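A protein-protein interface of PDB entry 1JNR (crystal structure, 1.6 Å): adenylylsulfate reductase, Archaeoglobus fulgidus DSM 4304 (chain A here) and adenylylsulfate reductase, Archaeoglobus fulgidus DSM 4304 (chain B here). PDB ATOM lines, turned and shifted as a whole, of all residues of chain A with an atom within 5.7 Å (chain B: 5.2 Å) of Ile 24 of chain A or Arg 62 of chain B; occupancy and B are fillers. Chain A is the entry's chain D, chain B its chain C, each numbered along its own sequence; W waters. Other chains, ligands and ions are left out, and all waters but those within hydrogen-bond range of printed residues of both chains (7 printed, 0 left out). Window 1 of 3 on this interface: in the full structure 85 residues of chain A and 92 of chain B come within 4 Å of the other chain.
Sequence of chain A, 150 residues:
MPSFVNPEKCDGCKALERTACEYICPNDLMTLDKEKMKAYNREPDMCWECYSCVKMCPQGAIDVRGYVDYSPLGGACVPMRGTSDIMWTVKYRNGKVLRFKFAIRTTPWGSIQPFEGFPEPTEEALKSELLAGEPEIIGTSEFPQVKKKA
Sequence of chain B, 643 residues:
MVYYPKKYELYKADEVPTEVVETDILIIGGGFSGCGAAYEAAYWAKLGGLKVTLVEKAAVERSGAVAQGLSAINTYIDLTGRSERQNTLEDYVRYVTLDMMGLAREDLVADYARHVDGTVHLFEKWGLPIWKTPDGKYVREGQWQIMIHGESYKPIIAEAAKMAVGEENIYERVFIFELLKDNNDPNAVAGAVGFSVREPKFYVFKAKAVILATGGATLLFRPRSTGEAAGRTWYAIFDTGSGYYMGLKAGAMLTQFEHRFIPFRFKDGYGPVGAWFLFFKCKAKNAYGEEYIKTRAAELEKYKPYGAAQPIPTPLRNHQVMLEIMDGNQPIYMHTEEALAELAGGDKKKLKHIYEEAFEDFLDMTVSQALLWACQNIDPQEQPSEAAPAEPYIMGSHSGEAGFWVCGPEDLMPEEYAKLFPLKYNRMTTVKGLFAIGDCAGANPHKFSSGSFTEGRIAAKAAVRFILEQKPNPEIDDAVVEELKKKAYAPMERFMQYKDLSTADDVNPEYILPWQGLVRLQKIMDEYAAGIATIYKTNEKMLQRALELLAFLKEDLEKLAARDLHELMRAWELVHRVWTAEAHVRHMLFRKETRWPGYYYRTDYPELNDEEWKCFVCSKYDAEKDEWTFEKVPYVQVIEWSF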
ATOM      1  N   THR A  19      28.826 -20.989 -17.977  1.00  0.00           N
ATOM      2  CA  THR A  19      28.223 -19.686 -17.721  1.00  0.00           C
ATOM      3  C   THR A  19      26.795 -19.934 -17.238  1.00  0.00           C
ATOM      4  O   THR A  19      25.945 -20.367 -18.011  1.00  0.00           O
ATOM      5  CB  THR A  19      28.202 -18.843 -19.009  1.00  0.00           C
ATOM      6  OG1 THR A  19      29.520 -18.808 -19.575  1.00  0.00           O
ATOM      7  CG2 THR A  19      27.755 -17.422 -18.712  1.00  0.00           C
ATOM      8  N   ALA A  20      26.545 -19.655 -15.962  1.00  0.00           N
ATOM      9  CA  ALA A  20      25.238 -19.896 -15.353  1.00  0.00           C
ATOM     10  C   ALA A  20      24.022 -19.270 -16.039  1.00  0.00           C
ATOM     11  O   ALA A  20      23.071 -19.978 -16.377  1.00  0.00           O
ATOM     12  CB  ALA A  20      25.271 -19.480 -13.881  1.00  0.00           C
ATOM     13  N   CYS A  21      24.042 -17.957 -16.240  1.00  0.00           N
ATOM     14  CA  CYS A  21      22.909 -17.277 -16.870  1.00  0.00           C
ATOM     15  C   CYS A  21      22.633 -17.767 -18.288  1.00  0.00           C
ATOM     16  O   CYS A  21      21.482 -17.995 -18.661  1.00  0.00           O
ATOM     17  CB  CYS A  21      23.127 -15.760 -16.877  1.00  0.00           C
ATOM     18  SG  CYS A  21      24.676 -15.212 -17.640  1.00  0.00           S
ATOM     19  N   GLU A  22      23.693 -17.922 -19.075  1.00  0.00           N
ATOM     20  CA  GLU A  22      23.565 -18.394 -20.448  1.00  0.00           C
ATOM     21  C   GLU A  22      22.965 -19.793 -20.449  1.00  0.00           C
ATOM     22  O   GLU A  22      22.118 -20.128 -21.275  1.00  0.00           O
ATOM     23  CB  GLU A  22      24.937 -18.439 -21.118  1.00  0.00           C
ATOM     24  CG  GLU A  22      24.905 -18.888 -22.565  1.00  0.00           C
ATOM     25  CD  GLU A  22      26.277 -19.283 -23.081  1.00  0.00           C
ATOM     26  OE1 GLU A  22      26.510 -19.167 -24.300  1.00  0.00           O
ATOM     27  OE2 GLU A  22      27.116 -19.727 -22.269  1.00  0.00           O
ATOM     28  N   TYR A  23      23.419 -20.608 -19.508  1.00  0.00           N
ATOM     29  CA  TYR A  23      22.947 -21.977 -19.388  1.00  0.00           C
ATOM     30  C   TYR A  23      21.479 -22.098 -19.001  1.00  0.00           C
ATOM     31  O   TYR A  23      20.750 -22.921 -19.554  1.00  0.00           O
ATOM     32  CB  TYR A  23      23.787 -22.718 -18.341  1.00  0.00           C
ATOM     33  CG  TYR A  23      23.063 -23.872 -17.679  1.00  0.00           C
ATOM     34  CD1 TYR A  23      22.846 -25.070 -18.357  1.00  0.00           C
ATOM     35  CD2 TYR A  23      22.555 -23.744 -16.387  1.00  0.00           C
ATOM     36  CE1 TYR A  23      22.134 -26.116 -17.762  1.00  0.00           C
ATOM     37  CE2 TYR A  23      21.842 -24.779 -15.785  1.00  0.00           C
ATOM     38  CZ  TYR A  23      21.635 -25.960 -16.476  1.00  0.00           C
ATOM     39  OH  TYR A  23      20.914 -26.975 -15.881  1.00  0.00           O
ATOM     40  N   ILE A  24      21.046 -21.267 -18.060  1.00  0.00           N
ATOM     41  CA  ILE A  24      19.687 -21.358 -17.534  1.00  0.00           C
ATOM     42  C   ILE A  24      18.527 -20.678 -18.266  1.00  0.00           C
ATOM     43  O   ILE A  24      17.407 -21.188 -18.233  1.00  0.00           O
ATOM     44  CB  ILE A  24      19.667 -20.881 -16.052  1.00  0.00           C
ATOM     45  CG1 ILE A  24      18.468 -21.480 -15.313  1.00  0.00           C
ATOM     46  CG2 ILE A  24      19.619 -19.359 -15.985  1.00  0.00           C
ATOM     47  CD1 ILE A  24      18.593 -22.970 -15.055  1.00  0.00           C
ATOM     48  N   CYS A  25      18.776 -19.547 -18.922  1.00  0.00           N
ATOM     49  CA  CYS A  25      17.691 -18.807 -19.579  1.00  0.00           C
ATOM     50  C   CYS A  25      16.798 -19.590 -20.540  1.00  0.00           C
ATOM     51  O   CYS A  25      17.238 -20.044 -21.592  1.00  0.00           O
ATOM     52  CB  CYS A  25      18.236 -17.579 -20.307  1.00  0.00           C
ATOM     53  SG  CYS A  25      16.915 -16.637 -21.106  1.00  0.00           S
ATOM     54  N   PRO A  26      15.504 -19.715 -20.200  1.00  0.00           N
ATOM     55  CA  PRO A  26      14.549 -20.447 -21.035  1.00  0.00           C
ATOM     56  C   PRO A  26      14.296 -19.864 -22.424  1.00  0.00           C
ATOM     57  O   PRO A  26      13.743 -20.549 -23.285  1.00  0.00           O
ATOM     58  CB  PRO A  26      13.277 -20.456 -20.187  1.00  0.00           C
ATOM     59  CG  PRO A  26      13.788 -20.319 -18.778  1.00  0.00           C
ATOM     60  CD  PRO A  26      14.876 -19.295 -18.936  1.00  0.00           C
ATOM     61  N   SER A  52      15.095 -16.606 -13.536  1.00  0.00           N
ATOM     62  CA  SER A  52      15.945 -17.794 -13.479  1.00  0.00           C
ATOM     63  C   SER A  52      17.420 -17.393 -13.451  1.00  0.00           C
ATOM     64  O   SER A  52      18.193 -17.899 -12.637  1.00  0.00           O
ATOM     65  CB  SER A  52      15.675 -18.719 -14.675  1.00  0.00           C
ATOM     66  OG  SER A  52      14.391 -19.327 -14.580  1.00  0.00           O
ATOM     67  N   CYS A  53      17.803 -16.480 -14.339  1.00  0.00           N
ATOM     68  CA  CYS A  53      19.186 -16.013 -14.403  1.00  0.00           C
ATOM     69  C   CYS A  53      19.580 -15.330 -13.095  1.00  0.00           C
ATOM     70  O   CYS A  53      20.681 -15.539 -12.581  1.00  0.00           O
ATOM     71  CB  CYS A  53      19.363 -15.036 -15.570  1.00  0.00           C
ATOM     72  SG  CYS A  53      18.251 -13.607 -15.539  1.00  0.00           S
ATOM     73  N   LYS A  55      18.367 -15.787 -10.050  1.00  0.00           N
ATOM     74  CA  LYS A  55      18.540 -16.779  -8.999  1.00  0.00           C
ATOM     75  C   LYS A  55      19.797 -17.638  -9.142  1.00  0.00           C
ATOM     76  O   LYS A  55      20.395 -18.033  -8.139  1.00  0.00           O
ATOM     77  CB  LYS A  55      17.322 -17.708  -8.949  1.00  0.00           C
ATOM     78  CG  LYS A  55      15.986 -17.027  -8.698  1.00  0.00           C
ATOM     79  CD  LYS A  55      14.848 -18.019  -8.883  1.00  0.00           C
ATOM     80  CE  LYS A  55      13.505 -17.382  -8.583  1.00  0.00           C
ATOM     81  NZ  LYS A  55      12.380 -18.290  -8.929  1.00  0.00           N
ATOM     82  N   MET A  56      20.201 -17.922 -10.378  1.00  0.00           N
ATOM     83  CA  MET A  56      21.352 -18.788 -10.602  1.00  0.00           C
ATOM     84  C   MET A  56      22.709 -18.113 -10.752  1.00  0.00           C
ATOM     85  O   MET A  56      23.725 -18.794 -10.893  1.00  0.00           O
ATOM     86  CB  MET A  56      21.092 -19.696 -11.810  1.00  0.00           C
ATOM     87  CG  MET A  56      19.801 -20.508 -11.703  1.00  0.00           C
ATOM     88  SD  MET A  56      19.517 -21.232 -10.061  1.00  0.00           S
ATOM     89  CE  MET A  56      20.699 -22.586 -10.072  1.00  0.00           C
ATOM     90  N   ARG A  81      18.226 -17.428  -3.100  1.00  0.00           N
ATOM     91  CA  ARG A  81      17.822 -18.823  -3.130  1.00  0.00           C
ATOM     92  C   ARG A  81      18.841 -19.776  -2.521  1.00  0.00           C
ATOM     93  O   ARG A  81      20.004 -19.801  -2.924  1.00  0.00           O
ATOM     94  CB  ARG A  81      17.523 -19.212  -4.580  1.00  0.00           C
ATOM     95  CG  ARG A  81      16.959 -20.603  -4.775  1.00  0.00           C
ATOM     96  CD  ARG A  81      16.327 -20.721  -6.155  1.00  0.00           C
ATOM     97  NE  ARG A  81      15.933 -22.091  -6.463  1.00  0.00           N
ATOM     98  CZ  ARG A  81      16.781 -23.054  -6.809  1.00  0.00           C
ATOM     99  NH1 ARG A  81      18.080 -22.802  -6.895  1.00  0.00           N
ATOM    100  NH2 ARG A  81      16.329 -24.274  -7.064  1.00  0.00           N
ATOM    101  N   ALA B  59      17.158 -25.263 -21.427  1.00  0.00           N
ATOM    102  CA  ALA B  59      17.717 -26.148 -20.400  1.00  0.00           C
ATOM    103  C   ALA B  59      16.577 -26.663 -19.520  1.00  0.00           C
ATOM    104  O   ALA B  59      15.854 -25.884 -18.899  1.00  0.00           O
ATOM    105  CB  ALA B  59      18.746 -25.400 -19.556  1.00  0.00           C
ATOM    106  N   VAL B  60      16.430 -27.982 -19.462  1.00  0.00           N
ATOM    107  CA  VAL B  60      15.355 -28.610 -18.701  1.00  0.00           C
ATOM    108  C   VAL B  60      15.176 -28.123 -17.263  1.00  0.00           C
ATOM    109  O   VAL B  60      14.054 -28.075 -16.761  1.00  0.00           O
ATOM    110  CB  VAL B  60      15.523 -30.148 -18.694  1.00  0.00           C
ATOM    111  CG1 VAL B  60      14.345 -30.799 -17.984  1.00  0.00           C
ATOM    112  CG2 VAL B  60      15.633 -30.661 -20.123  1.00  0.00           C
ATOM    113  N   GLU B  61      16.265 -27.756 -16.597  1.00  0.00           N
ATOM    114  CA  GLU B  61      16.162 -27.299 -15.215  1.00  0.00           C
ATOM    115  C   GLU B  61      15.105 -26.206 -15.005  1.00  0.00           C
ATOM    116  O   GLU B  61      14.428 -26.180 -13.973  1.00  0.00           O
ATOM    117  CB  GLU B  61      17.521 -26.794 -14.722  1.00  0.00           C
ATOM    118  CG  GLU B  61      17.522 -26.434 -13.248  1.00  0.00           C
ATOM    119  CD  GLU B  61      18.877 -25.972 -12.758  1.00  0.00           C
ATOM    120  OE1 GLU B  61      19.883 -26.251 -13.444  1.00  0.00           O
ATOM    121  OE2 GLU B  61      18.935 -25.346 -11.680  1.00  0.00           O
ATOM    122  N   ARG B  62      14.953 -25.313 -15.980  1.00  0.00           N
ATOM    123  CA  ARG B  62      13.990 -24.218 -15.857  1.00  0.00           C
ATOM    124  C   ARG B  62      13.152 -23.957 -17.102  1.00  0.00           C
ATOM    125  O   ARG B  62      12.392 -22.991 -17.138  1.00  0.00           O
ATOM    126  CB  ARG B  62      14.723 -22.917 -15.508  1.00  0.00           C
ATOM    127  CG  ARG B  62      15.275 -22.851 -14.099  1.00  0.00           C
ATOM    128  CD  ARG B  62      14.181 -22.527 -13.098  1.00  0.00           C
ATOM    129  NE  ARG B  62      14.697 -22.549 -11.734  1.00  0.00           N
ATOM    130  CZ  ARG B  62      14.017 -22.172 -10.658  1.00  0.00           C
ATOM    131  NH1 ARG B  62      12.770 -21.725 -10.769  1.00  0.00           N
ATOM    132  NH2 ARG B  62      14.581 -22.264  -9.459  1.00  0.00           N
ATOM    133  N   SER B  63      13.261 -24.810 -18.111  1.00  0.00           N
ATOM    134  CA  SER B  63      12.539 -24.562 -19.354  1.00  0.00           C
ATOM    135  C   SER B  63      11.020 -24.654 -19.285  1.00  0.00           C
ATOM    136  O   SER B  63      10.459 -25.396 -18.484  1.00  0.00           O
ATOM    137  CB  SER B  63      13.056 -25.491 -20.457  1.00  0.00           C
ATOM    138  OG  SER B  63      12.764 -26.851 -20.175  1.00  0.00           O
ATOM    139  N   GLY B  64      10.363 -23.870 -20.132  1.00  0.00           N
ATOM    140  CA  GLY B  64       8.914 -23.906 -20.188  1.00  0.00           C
ATOM    141  C   GLY B  64       8.126 -23.012 -19.253  1.00  0.00           C
ATOM    142  O   GLY B  64       8.662 -22.156 -18.549  1.00  0.00           O
ATOM    143  N   VAL B  66       6.853 -23.400 -16.393  1.00  0.00           N
ATOM    144  CA  VAL B  66       7.116 -23.434 -14.954  1.00  0.00           C
ATOM    145  C   VAL B  66       8.490 -22.878 -14.556  1.00  0.00           C
ATOM    146  O   VAL B  66       9.005 -23.157 -13.472  1.00  0.00           O
ATOM    147  CB  VAL B  66       6.941 -24.881 -14.430  1.00  0.00           C
ATOM    148  CG1 VAL B  66       6.996 -24.922 -12.901  1.00  0.00           C
ATOM    149  CG2 VAL B  66       5.602 -25.429 -14.919  1.00  0.00           C
ATOM    150  N   ALA B  67       9.059 -22.050 -15.423  1.00  0.00           N
ATOM    151  CA  ALA B  67      10.367 -21.451 -15.165  1.00  0.00           C
ATOM    152  C   ALA B  67      10.461 -20.687 -13.839  1.00  0.00           C
ATOM    153  O   ALA B  67      11.494 -20.736 -13.168  1.00  0.00           O
ATOM    154  CB  ALA B  67      10.747 -20.530 -16.320  1.00  0.00           C
ATOM    155  N   GLN B  68       9.401 -19.976 -13.462  1.00  0.00           N
ATOM    156  CA  GLN B  68       9.423 -19.208 -12.215  1.00  0.00           C
ATOM    157  C   GLN B  68       8.951 -20.049 -11.045  1.00  0.00           C
ATOM    158  O   GLN B  68       9.161 -19.690  -9.884  1.00  0.00           O
ATOM    159  CB  GLN B  68       8.502 -17.988 -12.308  1.00  0.00           C
ATOM    160  CG  GLN B  68       8.591 -17.208 -13.603  1.00  0.00           C
ATOM    161  CD  GLN B  68       7.900 -15.858 -13.521  1.00  0.00           C
ATOM    162  OE1 GLN B  68       7.344 -15.372 -14.509  1.00  0.00           O
ATOM    163  NE2 GLN B  68       7.943 -15.238 -12.347  1.00  0.00           N
ATOM    164  N   GLY B  69       8.325 -21.173 -11.375  1.00  0.00           N
ATOM    165  CA  GLY B  69       7.751 -22.060 -10.386  1.00  0.00           C
ATOM    166  C   GLY B  69       6.254 -21.834 -10.524  1.00  0.00           C
ATOM    167  O   GLY B  69       5.830 -21.127 -11.438  1.00  0.00           O
ATOM    168  N   GLU B 151       8.513 -22.716  -5.900  1.00  0.00           N
ATOM    169  CA  GLU B 151       9.549 -21.972  -6.600  1.00  0.00           C
ATOM    170  C   GLU B 151      10.462 -22.899  -7.407  1.00  0.00           C
ATOM    171  O   GLU B 151      10.879 -22.557  -8.512  1.00  0.00           O
ATOM    172  CB  GLU B 151      10.386 -21.159  -5.607  1.00  0.00           C
ATOM    173  CG  GLU B 151      11.418 -20.244  -6.267  1.00  0.00           C
ATOM    174  CD  GLU B 151      12.700 -20.961  -6.669  1.00  0.00           C
ATOM    175  OE1 GLU B 151      13.322 -20.546  -7.672  1.00  0.00           O
ATOM    176  OE2 GLU B 151      13.097 -21.925  -5.975  1.00  0.00           O
ATOM    177  N   SER B 152      10.759 -24.075  -6.857  1.00  0.00           N
ATOM    178  CA  SER B 152      11.634 -25.038  -7.526  1.00  0.00           C
ATOM    179  C   SER B 152      10.891 -26.203  -8.168  1.00  0.00           C
ATOM    180  O   SER B 152      11.466 -27.268  -8.397  1.00  0.00           O
ATOM    181  CB  SER B 152      12.665 -25.584  -6.531  1.00  0.00           C
ATOM    182  OG  SER B 152      13.573 -24.567  -6.147  1.00  0.00           O
ATOM    183  N   LYS B 154       9.891 -26.796 -11.245  1.00  0.00           N
ATOM    184  CA  LYS B 154      10.502 -27.325 -12.460  1.00  0.00           C
ATOM    185  C   LYS B 154      11.846 -28.015 -12.193  1.00  0.00           C
ATOM    186  O   LYS B 154      12.091 -29.100 -12.711  1.00  0.00           O
ATOM    187  CB  LYS B 154      10.669 -26.224 -13.519  1.00  0.00           C
ATOM    188  CG  LYS B 154      11.153 -26.760 -14.876  1.00  0.00           C
ATOM    189  CD  LYS B 154      10.156 -27.768 -15.481  1.00  0.00           C
ATOM    190  CE  LYS B 154      10.800 -28.665 -16.544  1.00  0.00           C
ATOM    191  NZ  LYS B 154      11.423 -27.921 -17.682  1.00  0.00           N
ATOM    192  N   PRO B 155      12.735 -27.402 -11.389  1.00  0.00           N
ATOM    193  CA  PRO B 155      14.019 -28.070 -11.129  1.00  0.00           C
ATOM    194  C   PRO B 155      13.837 -29.458 -10.512  1.00  0.00           C
ATOM    195  O   PRO B 155      14.591 -30.390 -10.811  1.00  0.00           O
ATOM    196  CB  PRO B 155      14.724 -27.103 -10.184  1.00  0.00           C
ATOM    197  CG  PRO B 155      14.232 -25.770 -10.658  1.00  0.00           C
ATOM    198  CD  PRO B 155      12.750 -26.021 -10.876  1.00  0.00           C
ATOM    199  N   ARG B 173      19.630 -27.143 -25.684  1.00  0.00           N
ATOM    200  CA  ARG B 173      19.983 -26.086 -26.621  1.00  0.00           C
ATOM    201  C   ARG B 173      19.953 -26.579 -28.067  1.00  0.00           C
ATOM    202  O   ARG B 173      20.775 -26.193 -28.898  1.00  0.00           O
ATOM    203  CB  ARG B 173      21.348 -25.476 -26.270  1.00  0.00           C
ATOM    204  CG  ARG B 173      21.366 -24.774 -24.913  1.00  0.00           C
ATOM    205  CD  ARG B 173      20.340 -23.634 -24.820  1.00  0.00           C
ATOM    206  NE  ARG B 173      20.179 -23.181 -23.438  1.00  0.00           N
ATOM    207  CZ  ARG B 173      19.371 -22.198 -23.046  1.00  0.00           C
ATOM    208  NH1 ARG B 173      18.630 -21.538 -23.926  1.00  0.00           N
ATOM    209  NH2 ARG B 173      19.305 -21.878 -21.763  1.00  0.00           N
HETATM  210  O   HOH W   1       9.895 -17.415  -8.514  1.00  0.00           O
HETATM  211  O   HOH W   2      19.030 -28.415 -17.286  1.00  0.00           O
HETATM  212  O   HOH W   3      12.974 -18.520 -11.811  1.00  0.00           O
HETATM  213  O   HOH W   4      11.946 -22.741 -22.317  1.00  0.00           O
HETATM  214  O   HOH W   5      15.925 -23.117 -19.659  1.00  0.00           O
HETATM  215  O   HOH W   6      21.783 -24.411 -21.500  1.00  0.00           O
HETATM  216  O   HOH W   7      17.156 -23.441 -10.714  1.00  0.00           O
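Among the printed residues, merely in contact across the chains: Tyr 23 of chain A with Ala 59 of chain B (3.2 Å), Ile 24 of chain A with Glu 61 of chain B (3.8 Å), Ile 24 of chain A with Arg 62 of chain B (3.5 Å), Ile 24 of chain A with Arg 173 of chain B (3.8 Å), Pro 26 of chain A with Arg 62 of chain B (3.4 Å), Pro 26 of chain A with Ala 67 of chain B (3.9 Å), Ser 52 of chain A with Arg 62 of chain B (3.5 Å), Ser 52 of chain A with Ala 67 of chain B (3.5 Å), Lys 55 of chain A with Arg 62 of chain B (3.9 Å), Lys 55 of chain A with Gln 68 of chain B (3.6 Å) and Met 56 of chain A with Glu 61 of chain B (3.6 Å).
The side-chain carboxylate of Glu 61 of chain B is in hydrogen-bond range of the side-chain hydroxyl of Tyr 23 of chain A. The side-chain amino group (NZ) of Lys 55 of chain A is in salt-bridge range of the side-chain carboxylate (OE1) of Glu 151 of chain B (2.7 Å). The guanidinium group (NE) of Arg 81 of chain A lies within salt-bridge range of the side-chain carboxylate (OE2) of Glu 151 of chain B (2.9 Å). OG of Ser 152 of chain B lies within hydrogen-bond range of NH2 of Arg 81 of chain A, 2.9 Å away. The guanidinium group (NH2) of Arg 173 of chain B is in hydrogen-bond range of the backbone carbonyl oxygen (O) of Glu 22 of chain A (3.3 Å). The guanidinium group of Arg 173 of chain B lies within hydrogen-bond range of the backbone carbonyl oxygen of Tyr 23 of chain A (2.8 Å). NH2 of Arg 173 of chain B lies within hydrogen-bond range of O of Cys 25 of chain A (2.8 Å). The guanidinium group (NE) of Arg 81 of chain A lies close to the guanidinium group (NH2) of Arg 62 of chain B (3.3 Å).
Of the printed residues of chain B, Ile 24 of chain A touches Glu 61, Arg 62 and Arg 173. Arg 62 of chain B touches just these residues of chain A: Ile 24, Pro 26, Ser 52, Lys 55 and Arg 81. Printed residues of chain B within 4 Å of Tyr 23 of chain A: Ala 59, Glu 61 and Arg 173. Of the printed residues of chain B, Arg 81 of chain A touches Arg 62, Glu 151 and Ser 152. Of the printed residues of chain A, Glu 151 of chain B touches Lys 55 and Arg 81. Printed residues of chain A within 4 Å of Gln 68 of chain B: Lys 55. Of the printed residues of chain B, Met 56 of chain A touches Glu 61. The nearest printed residue of chain A that does not touch Gln 68 of chain B is Ser 52 of chain A (5.2 Å).
Water W6 lies within hydrogen-bond range of O of Tyr 23 of chain A and NE of Arg 173 of chain B. Water W1 bridges NZ of Lys 55 of chain A (2.7 Å) and O of Gln 68 of chain B (2.8 Å). Water W2 lies within hydrogen-bond range of OH of Tyr 23 of chain A (2.8 Å), N of Glu 61 of chain B (2.9 Å) and N of Val 60 of chain B (3.4 Å). Water W7 lies within hydrogen-bond range of OE2 of Glu 61 of chain B (2.8 Å), NE of Arg 62 of chain B (2.8 Å) and SD of Met 56 of chain A (3.3 Å). Water W4 bridges N of Gly 64 of chain B and O of Pro 26 of chain A. Water W3 lies within hydrogen-bond range of NZ of Lys 55 of chain A (3.0 Å), O of Ala 67 of chain B (3.0 Å), OG of Ser 52 of chain A (3.2 Å) and NH1 of Arg 62 of chain B (3.4 Å).
The side-chain hydroxyl of Ser 63 of chain B sits close to the backbone carbonyl oxygen of Ala 59 of chain B. O of Ala 67 of chain B lies within hydrogen-bond range of NH1 of Arg 62 of chain B, at 2.9 Å. NH2 of Arg 62 of chain B is in salt-bridge range of OE1 of Glu 151 of chain B (2.8 Å). OG of Ser 152 of chain B lies within hydrogen-bond range of OE2 of Glu 151 of chain B, 2.7 Å away.
Of the 13 printed residues of chain A, 9 touch a printed residue of chain B. Printed residues of chain A that touch a printed residue of chain B: Glu 22, Tyr 23, Ile 24, Cys 25, Pro 26, Ser 52, Lys 55, Met 56 and Arg 81. Hydrophobic or aromatic side chains of chain B that line the printed part of chain A: Ala 59 and Ala 67. Along chain B the printed residues that touch a printed residue of chain A span positions 59 to 173.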
